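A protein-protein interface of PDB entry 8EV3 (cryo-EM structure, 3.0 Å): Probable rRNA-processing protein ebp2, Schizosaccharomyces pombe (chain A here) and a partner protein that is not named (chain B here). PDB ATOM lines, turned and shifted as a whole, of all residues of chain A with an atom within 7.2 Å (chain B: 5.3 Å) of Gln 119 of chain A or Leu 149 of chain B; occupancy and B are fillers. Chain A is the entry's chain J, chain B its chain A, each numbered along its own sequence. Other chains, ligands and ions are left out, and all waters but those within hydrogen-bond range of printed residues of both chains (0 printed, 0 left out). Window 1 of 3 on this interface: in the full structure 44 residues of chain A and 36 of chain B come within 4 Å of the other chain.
Of the 14 printed residues of chain B, 7 touch a printed residue of chain A. Hydrophobic or aromatic side chains of chain B that line the printed part of chain A: Ile 148 and Leu 149. Hydrophobic or aromatic side chains of chain A that line the printed part of chain B: Ala 120, Val 121 and Ala 153. Among the printed residues, 18 pairs touch across the chains.
The backbone carbonyl oxygen (O) of Phe 115 of chain A sits at hydrogen-bond distance from the backbone NH (N) of Ala 120 of chain A (3.1 Å). The backbone carbonyl oxygen (O) of Ile 174 of chain B is in hydrogen-bond range of the guanidinium group (NE) of Arg 146 of chain B, at 3.3 Å. O of Ile 148 of chain B lies within hydrogen-bond range of N of Cys 189 of chain B, 2.5 Å away. O of Cys 189 of chain B sits at hydrogen-bond distance from N of Ser 150 of chain B, at 2.5 Å. The backbone carbonyl oxygen (O) of Ser 150 of chain B lies within hydrogen-bond range of the backbone NH (N) of Leu 191 of chain B, 2.7 Å away.
The backbone carbonyl oxygen (O) of Val 116 of chain A sits at hydrogen-bond distance from the guanidinium group (NH1) of Arg 146 of chain B. The guanidinium group of Arg 146 of chain B lies within hydrogen-bond range of the backbone carbonyl oxygen of Glu 117 of chain A, 2.4 Å away. O of Gln 119 of chain A lies within hydrogen-bond range of N of Leu 149 of chain B (3.2 Å). The backbone NH (N) of Val 121 of chain A lies within hydrogen-bond range of the backbone carbonyl oxygen (O) of Leu 149 of chain B (2.9 Å). The backbone NH (N) of Gln 119 of chain A sits close to the guanidinium group (NH2) of Arg 146 of chain B (3.5 Å). The backbone carbonyl oxygen (O) of Gln 119 of chain A lies close to the backbone carbonyl oxygen (O) of Pro 147 of chain B.
Among the printed residues, pairs that only touch across the chains: Val 121 of chain A with Ser 150 of chain B (3.1 Å), Ala 120 of chain A with Leu 149 of chain B (3.4 Å), Thr 122 of chain A with Phe 151 of chain B (3.5 Å), Ala 120 of chain A with Gln 169 of chain B (3.6 Å), Ala 153 of chain A with Ile 148 of chain B (3.6 Å), Asn 118 of chain A with Arg 146 of chain B (3.7 Å), Thr 123 of chain A with Ser 150 of chain B (3.7 Å), Val 121 of chain A with Ile 148 of chain B (3.7 Å), Gln 119 of chain A with Ile 148 of chain B (3.7 Å), Thr 122 of chain A with Ser 150 of chain B (3.7 Å), Thr 123 of chain A with Phe 151 of chain B (3.8 Å) and Thr 122 of chain A with Leu 149 of chain B (3.9 Å).
Printed residues of chain B within 4 Å of Thr 123 of chain A: Ser 150 (3.7 Å) and Phe 151 (3.8 Å). Of the printed residues of chain B, Asn 118 of chain A touches Arg 146. Printed residues of chain B within 4 Å of Val 116 of chain A: Arg 146 (2.4 Å).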
ATOM      1  N   ILE A 113      12.873  -7.038 -31.516  1.00  0.00           N
ATOM      2  CA  ILE A 113      12.629  -8.373 -30.986  1.00  0.00           C
ATOM      3  C   ILE A 113      11.278  -8.869 -31.475  1.00  0.00           C
ATOM      4  O   ILE A 113      10.263  -8.167 -31.371  1.00  0.00           O
ATOM      5  CB  ILE A 113      12.706  -8.363 -29.453  1.00  0.00           C
ATOM      6  N   SER A 114      11.260 -10.084 -32.016  1.00  0.00           N
ATOM      7  CA  SER A 114      10.040 -10.643 -32.573  1.00  0.00           C
ATOM      8  C   SER A 114       9.035 -10.949 -31.463  1.00  0.00           C
ATOM      9  O   SER A 114       9.340 -10.885 -30.269  1.00  0.00           O
ATOM     10  CB  SER A 114      10.347 -11.906 -33.376  1.00  0.00           C
ATOM     11  N   PHE A 115       7.812 -11.288 -31.880  1.00  0.00           N
ATOM     12  CA  PHE A 115       6.770 -11.621 -30.916  1.00  0.00           C
ATOM     13  C   PHE A 115       7.163 -12.832 -30.079  1.00  0.00           C
ATOM     14  O   PHE A 115       6.957 -12.847 -28.860  1.00  0.00           O
ATOM     15  CB  PHE A 115       5.448 -11.874 -31.638  1.00  0.00           C
ATOM     16  N   VAL A 116       7.729 -13.858 -30.717  1.00  0.00           N
ATOM     17  CA  VAL A 116       8.242 -14.999 -29.968  1.00  0.00           C
ATOM     18  C   VAL A 116       9.494 -14.609 -29.193  1.00  0.00           C
ATOM     19  O   VAL A 116       9.683 -15.025 -28.043  1.00  0.00           O
ATOM     20  CB  VAL A 116       8.508 -16.183 -30.914  1.00  0.00           C
ATOM     21  N   GLU A 117      10.370 -13.811 -29.810  1.00  0.00           N
ATOM     22  CA  GLU A 117      11.609 -13.411 -29.148  1.00  0.00           C
ATOM     23  C   GLU A 117      11.332 -12.536 -27.932  1.00  0.00           C
ATOM     24  O   GLU A 117      11.898 -12.756 -26.854  1.00  0.00           O
ATOM     25  CB  GLU A 117      12.519 -12.684 -30.140  1.00  0.00           C
ATOM     26  N   ASN A 118      10.464 -11.539 -28.083  1.00  0.00           N
ATOM     27  CA  ASN A 118      10.114 -10.643 -26.988  1.00  0.00           C
ATOM     28  C   ASN A 118       9.001 -11.193 -26.107  1.00  0.00           C
ATOM     29  O   ASN A 118       8.679 -10.571 -25.088  1.00  0.00           O
ATOM     30  CB  ASN A 118       9.705  -9.271 -27.534  1.00  0.00           C
ATOM     31  N   GLN A 119       8.416 -12.335 -26.472  1.00  0.00           N
ATOM     32  CA  GLN A 119       7.348 -12.966 -25.696  1.00  0.00           C
ATOM     33  C   GLN A 119       6.178 -12.008 -25.475  1.00  0.00           C
ATOM     34  O   GLN A 119       5.596 -11.949 -24.391  1.00  0.00           O
ATOM     35  CB  GLN A 119       7.877 -13.496 -24.362  1.00  0.00           C
ATOM     36  N   ALA A 120       5.830 -11.249 -26.512  1.00  0.00           N
ATOM     37  CA  ALA A 120       4.740 -10.281 -26.409  1.00  0.00           C
ATOM     38  C   ALA A 120       4.192 -10.009 -27.798  1.00  0.00           C
ATOM     39  O   ALA A 120       4.932  -9.553 -28.677  1.00  0.00           O
ATOM     40  CB  ALA A 120       5.221  -8.986 -25.754  1.00  0.00           C
ATOM     41  N   VAL A 121       2.905 -10.285 -27.997  1.00  0.00           N
ATOM     42  CA  VAL A 121       2.232 -10.001 -29.259  1.00  0.00           C
ATOM     43  C   VAL A 121       0.853  -9.433 -28.959  1.00  0.00           C
ATOM     44  O   VAL A 121      -0.059 -10.170 -28.571  1.00  0.00           O
ATOM     45  CB  VAL A 121       2.134 -11.258 -30.142  1.00  0.00           C
ATOM     46  N   THR A 122       0.691  -8.125 -29.144  1.00  0.00           N
ATOM     47  CA  THR A 122      -0.556  -7.463 -28.791  1.00  0.00           C
ATOM     48  C   THR A 122      -1.705  -7.967 -29.657  1.00  0.00           C
ATOM     49  O   THR A 122      -1.508  -8.439 -30.779  1.00  0.00           O
ATOM     50  CB  THR A 122      -0.419  -5.947 -28.940  1.00  0.00           C
ATOM     51  N   THR A 123      -2.917  -7.873 -29.112  1.00  0.00           N
ATOM     52  CA  THR A 123      -4.101  -8.332 -29.825  1.00  0.00           C
ATOM     53  C   THR A 123      -4.292  -7.545 -31.116  1.00  0.00           C
ATOM     54  O   THR A 123      -4.071  -6.331 -31.162  1.00  0.00           O
ATOM     55  CB  THR A 123      -5.341  -8.196 -28.940  1.00  0.00           C
ATOM     56  N   ALA A 153      -0.435 -15.296 -32.778  1.00  0.00           N
ATOM     57  CA  ALA A 153       0.929 -15.315 -32.263  1.00  0.00           C
ATOM     58  C   ALA A 153       1.530 -16.713 -32.340  1.00  0.00           C
ATOM     59  O   ALA A 153       2.733 -16.863 -32.581  1.00  0.00           O
ATOM     60  CB  ALA A 153       0.956 -14.796 -30.826  1.00  0.00           C
ATOM     61  N   ARG B 146       7.717 -19.154 -21.587  1.00  0.00           N
ATOM     62  CA  ARG B 146       7.631 -17.748 -21.960  1.00  0.00           C
ATOM     63  C   ARG B 146       6.241 -17.424 -22.493  1.00  0.00           C
ATOM     64  O   ARG B 146       5.871 -17.874 -23.585  1.00  0.00           O
ATOM     65  CB  ARG B 146       8.697 -17.406 -23.000  1.00  0.00           C
ATOM     66  CG  ARG B 146      10.105 -17.765 -22.570  1.00  0.00           C
ATOM     67  CD  ARG B 146      11.119 -17.446 -23.654  1.00  0.00           C
ATOM     68  NE  ARG B 146      11.282 -16.010 -23.853  1.00  0.00           N
ATOM     69  CZ  ARG B 146      10.830 -15.343 -24.907  1.00  0.00           C
ATOM     70  NH1 ARG B 146      10.160 -15.949 -25.873  1.00  0.00           N
ATOM     71  NH2 ARG B 146      11.062 -14.037 -24.995  1.00  0.00           N
ATOM     72  N   PRO B 147       5.449 -16.650 -21.760  1.00  0.00           N
ATOM     73  CA  PRO B 147       4.099 -16.323 -22.218  1.00  0.00           C
ATOM     74  C   PRO B 147       4.119 -15.297 -23.341  1.00  0.00           C
ATOM     75  O   PRO B 147       5.071 -14.537 -23.514  1.00  0.00           O
ATOM     76  CB  PRO B 147       3.431 -15.748 -20.965  1.00  0.00           C
ATOM     77  CG  PRO B 147       4.554 -15.159 -20.186  1.00  0.00           C
ATOM     78  CD  PRO B 147       5.799 -15.948 -20.512  1.00  0.00           C
ATOM     79  N   ILE B 148       3.036 -15.290 -24.108  1.00  0.00           N
ATOM     80  CA  ILE B 148       2.818 -14.294 -25.149  1.00  0.00           C
ATOM     81  C   ILE B 148       1.878 -13.244 -24.575  1.00  0.00           C
ATOM     82  O   ILE B 148       0.701 -13.522 -24.320  1.00  0.00           O
ATOM     83  CB  ILE B 148       2.250 -14.920 -26.428  1.00  0.00           C
ATOM     84  CG1 ILE B 148       3.185 -16.018 -26.940  1.00  0.00           C
ATOM     85  CG2 ILE B 148       2.043 -13.854 -27.488  1.00  0.00           C
ATOM     86  CD1 ILE B 148       2.662 -16.744 -28.158  1.00  0.00           C
ATOM     87  N   LEU B 149       2.390 -12.037 -24.365  1.00  0.00           N
ATOM     88  CA  LEU B 149       1.631 -10.983 -23.709  1.00  0.00           C
ATOM     89  C   LEU B 149       0.932 -10.129 -24.759  1.00  0.00           C
ATOM     90  O   LEU B 149       1.589  -9.462 -25.564  1.00  0.00           O
ATOM     91  CB  LEU B 149       2.540 -10.128 -22.828  1.00  0.00           C
ATOM     92  CG  LEU B 149       2.881 -10.738 -21.464  1.00  0.00           C
ATOM     93  CD1 LEU B 149       3.975 -11.788 -21.577  1.00  0.00           C
ATOM     94  CD2 LEU B 149       3.258  -9.670 -20.457  1.00  0.00           C
ATOM     95  N   SER B 150      -0.397 -10.154 -24.747  1.00  0.00           N
ATOM     96  CA  SER B 150      -1.217  -9.359 -25.651  1.00  0.00           C
ATOM     97  C   SER B 150      -1.877  -8.244 -24.854  1.00  0.00           C
ATOM     98  O   SER B 150      -2.605  -8.513 -23.891  1.00  0.00           O
ATOM     99  CB  SER B 150      -2.268 -10.224 -26.347  1.00  0.00           C
ATOM    100  OG  SER B 150      -3.056 -10.929 -25.407  1.00  0.00           O
ATOM    101  N   PHE B 151      -1.623  -7.004 -25.252  1.00  0.00           N
ATOM    102  CA  PHE B 151      -2.168  -5.833 -24.582  1.00  0.00           C
ATOM    103  C   PHE B 151      -3.177  -5.156 -25.498  1.00  0.00           C
ATOM    104  O   PHE B 151      -2.921  -4.988 -26.695  1.00  0.00           O
ATOM    105  CB  PHE B 151      -1.059  -4.852 -24.197  1.00  0.00           C
ATOM    106  CG  PHE B 151      -0.179  -5.338 -23.081  1.00  0.00           C
ATOM    107  CD1 PHE B 151       0.833  -6.252 -23.326  1.00  0.00           C
ATOM    108  CD2 PHE B 151      -0.366  -4.885 -21.787  1.00  0.00           C
ATOM    109  CE1 PHE B 151       1.644  -6.700 -22.301  1.00  0.00           C
ATOM    110  CE2 PHE B 151       0.440  -5.331 -20.758  1.00  0.00           C
ATOM    111  CZ  PHE B 151       1.447  -6.240 -21.016  1.00  0.00           C
ATOM    112  N   LEU B 168       4.274  -3.776 -17.082  1.00  0.00           N
ATOM    113  CA  LEU B 168       3.572  -5.048 -16.954  1.00  0.00           C
ATOM    114  C   LEU B 168       4.136  -6.086 -17.915  1.00  0.00           C
ATOM    115  O   LEU B 168       4.250  -7.268 -17.570  1.00  0.00           O
ATOM    116  CB  LEU B 168       2.077  -4.847 -17.198  1.00  0.00           C
ATOM    117  CG  LEU B 168       1.121  -5.815 -16.503  1.00  0.00           C
ATOM    118  CD1 LEU B 168       1.065  -5.521 -15.015  1.00  0.00           C
ATOM    119  CD2 LEU B 168      -0.265  -5.731 -17.121  1.00  0.00           C
ATOM    120  N   GLN B 169       4.492  -5.663 -19.130  1.00  0.00           N
ATOM    121  CA  GLN B 169       4.994  -6.601 -20.129  1.00  0.00           C
ATOM    122  C   GLN B 169       6.358  -7.153 -19.733  1.00  0.00           C
ATOM    123  O   GLN B 169       6.598  -8.363 -19.821  1.00  0.00           O
ATOM    124  CB  GLN B 169       5.060  -5.923 -21.497  1.00  0.00           C
ATOM    125  CG  GLN B 169       6.214  -6.379 -22.376  1.00  0.00           C
ATOM    126  CD  GLN B 169       6.437  -5.465 -23.563  1.00  0.00           C
ATOM    127  OE1 GLN B 169       6.176  -4.263 -23.494  1.00  0.00           O
ATOM    128  NE2 GLN B 169       6.926  -6.029 -24.661  1.00  0.00           N
ATOM    129  N   PHE B 172       5.894  -9.496 -16.231  1.00  0.00           N
ATOM    130  CA  PHE B 172       5.146 -10.740 -16.388  1.00  0.00           C
ATOM    131  C   PHE B 172       5.760 -11.623 -17.467  1.00  0.00           C
ATOM    132  O   PHE B 172       5.803 -12.850 -17.321  1.00  0.00           O
ATOM    133  CB  PHE B 172       3.681 -10.438 -16.700  1.00  0.00           C
ATOM    134  CG  PHE B 172       2.878 -10.043 -15.493  1.00  0.00           C
ATOM    135  CD1 PHE B 172       3.167  -8.879 -14.802  1.00  0.00           C
ATOM    136  CD2 PHE B 172       1.846 -10.846 -15.038  1.00  0.00           C
ATOM    137  CE1 PHE B 172       2.435  -8.515 -13.689  1.00  0.00           C
ATOM    138  CE2 PHE B 172       1.112 -10.487 -13.924  1.00  0.00           C
ATOM    139  CZ  PHE B 172       1.406  -9.320 -13.250  1.00  0.00           C
ATOM    140  N   GLY B 173       6.230 -11.023 -18.557  1.00  0.00           N
ATOM    141  CA  GLY B 173       6.932 -11.769 -19.580  1.00  0.00           C
ATOM    142  C   GLY B 173       8.218 -12.379 -19.063  1.00  0.00           C
ATOM    143  O   GLY B 173       9.053 -11.678 -18.485  1.00  0.00           O
ATOM    144  N   ILE B 174       8.390 -13.682 -19.263  1.00  0.00           N
ATOM    145  CA  ILE B 174       9.562 -14.403 -18.774  1.00  0.00           C
ATOM    146  C   ILE B 174      10.671 -14.240 -19.810  1.00  0.00           C
ATOM    147  O   ILE B 174      10.533 -14.757 -20.931  1.00  0.00           O
ATOM    148  CB  ILE B 174       9.248 -15.883 -18.526  1.00  0.00           C
ATOM    149  CG1 ILE B 174       8.039 -16.020 -17.596  1.00  0.00           C
ATOM    150  CG2 ILE B 174      10.457 -16.593 -17.940  1.00  0.00           C
ATOM    151  CD1 ILE B 174       7.591 -17.447 -17.383  1.00  0.00           C
ATOM    152  N   VAL B 188      -0.492 -17.617 -22.797  1.00  0.00           N
ATOM    153  CA  VAL B 188      -0.604 -16.372 -23.552  1.00  0.00           C
ATOM    154  C   VAL B 188      -1.309 -15.355 -22.663  1.00  0.00           C
ATOM    155  O   VAL B 188      -2.461 -15.567 -22.270  1.00  0.00           O
ATOM    156  CB  VAL B 188      -1.364 -16.553 -24.873  1.00  0.00           C
ATOM    157  CG1 VAL B 188      -1.757 -15.203 -25.452  1.00  0.00           C
ATOM    158  CG2 VAL B 188      -0.521 -17.339 -25.867  1.00  0.00           C
ATOM    159  N   CYS B 189      -0.628 -14.255 -22.352  1.00  0.00           N
ATOM    160  CA  CYS B 189      -1.205 -13.225 -21.500  1.00  0.00           C
ATOM    161  C   CYS B 189      -2.062 -12.274 -22.326  1.00  0.00           C
ATOM    162  O   CYS B 189      -1.640 -11.805 -23.387  1.00  0.00           O
ATOM    163  CB  CYS B 189      -0.106 -12.444 -20.782  1.00  0.00           C
ATOM    164  SG  CYS B 189       0.996 -13.441 -19.758  1.00  0.00           S
ATOM    165  N   LEU B 191      -4.169  -8.705 -21.758  1.00  0.00           N
ATOM    166  CA  LEU B 191      -4.340  -7.574 -20.858  1.00  0.00           C
ATOM    167  C   LEU B 191      -5.231  -6.524 -21.505  1.00  0.00           C
ATOM    168  O   LEU B 191      -5.143  -6.279 -22.713  1.00  0.00           O
ATOM    169  CB  LEU B 191      -2.991  -6.951 -20.477  1.00  0.00           C
ATOM    170  CG  LEU B 191      -1.990  -7.817 -19.708  1.00  0.00           C
ATOM    171  CD1 LEU B 191      -2.713  -8.654 -18.661  1.00  0.00           C
ATOM    172  CD2 LEU B 191      -1.157  -8.693 -20.636  1.00  0.00           C
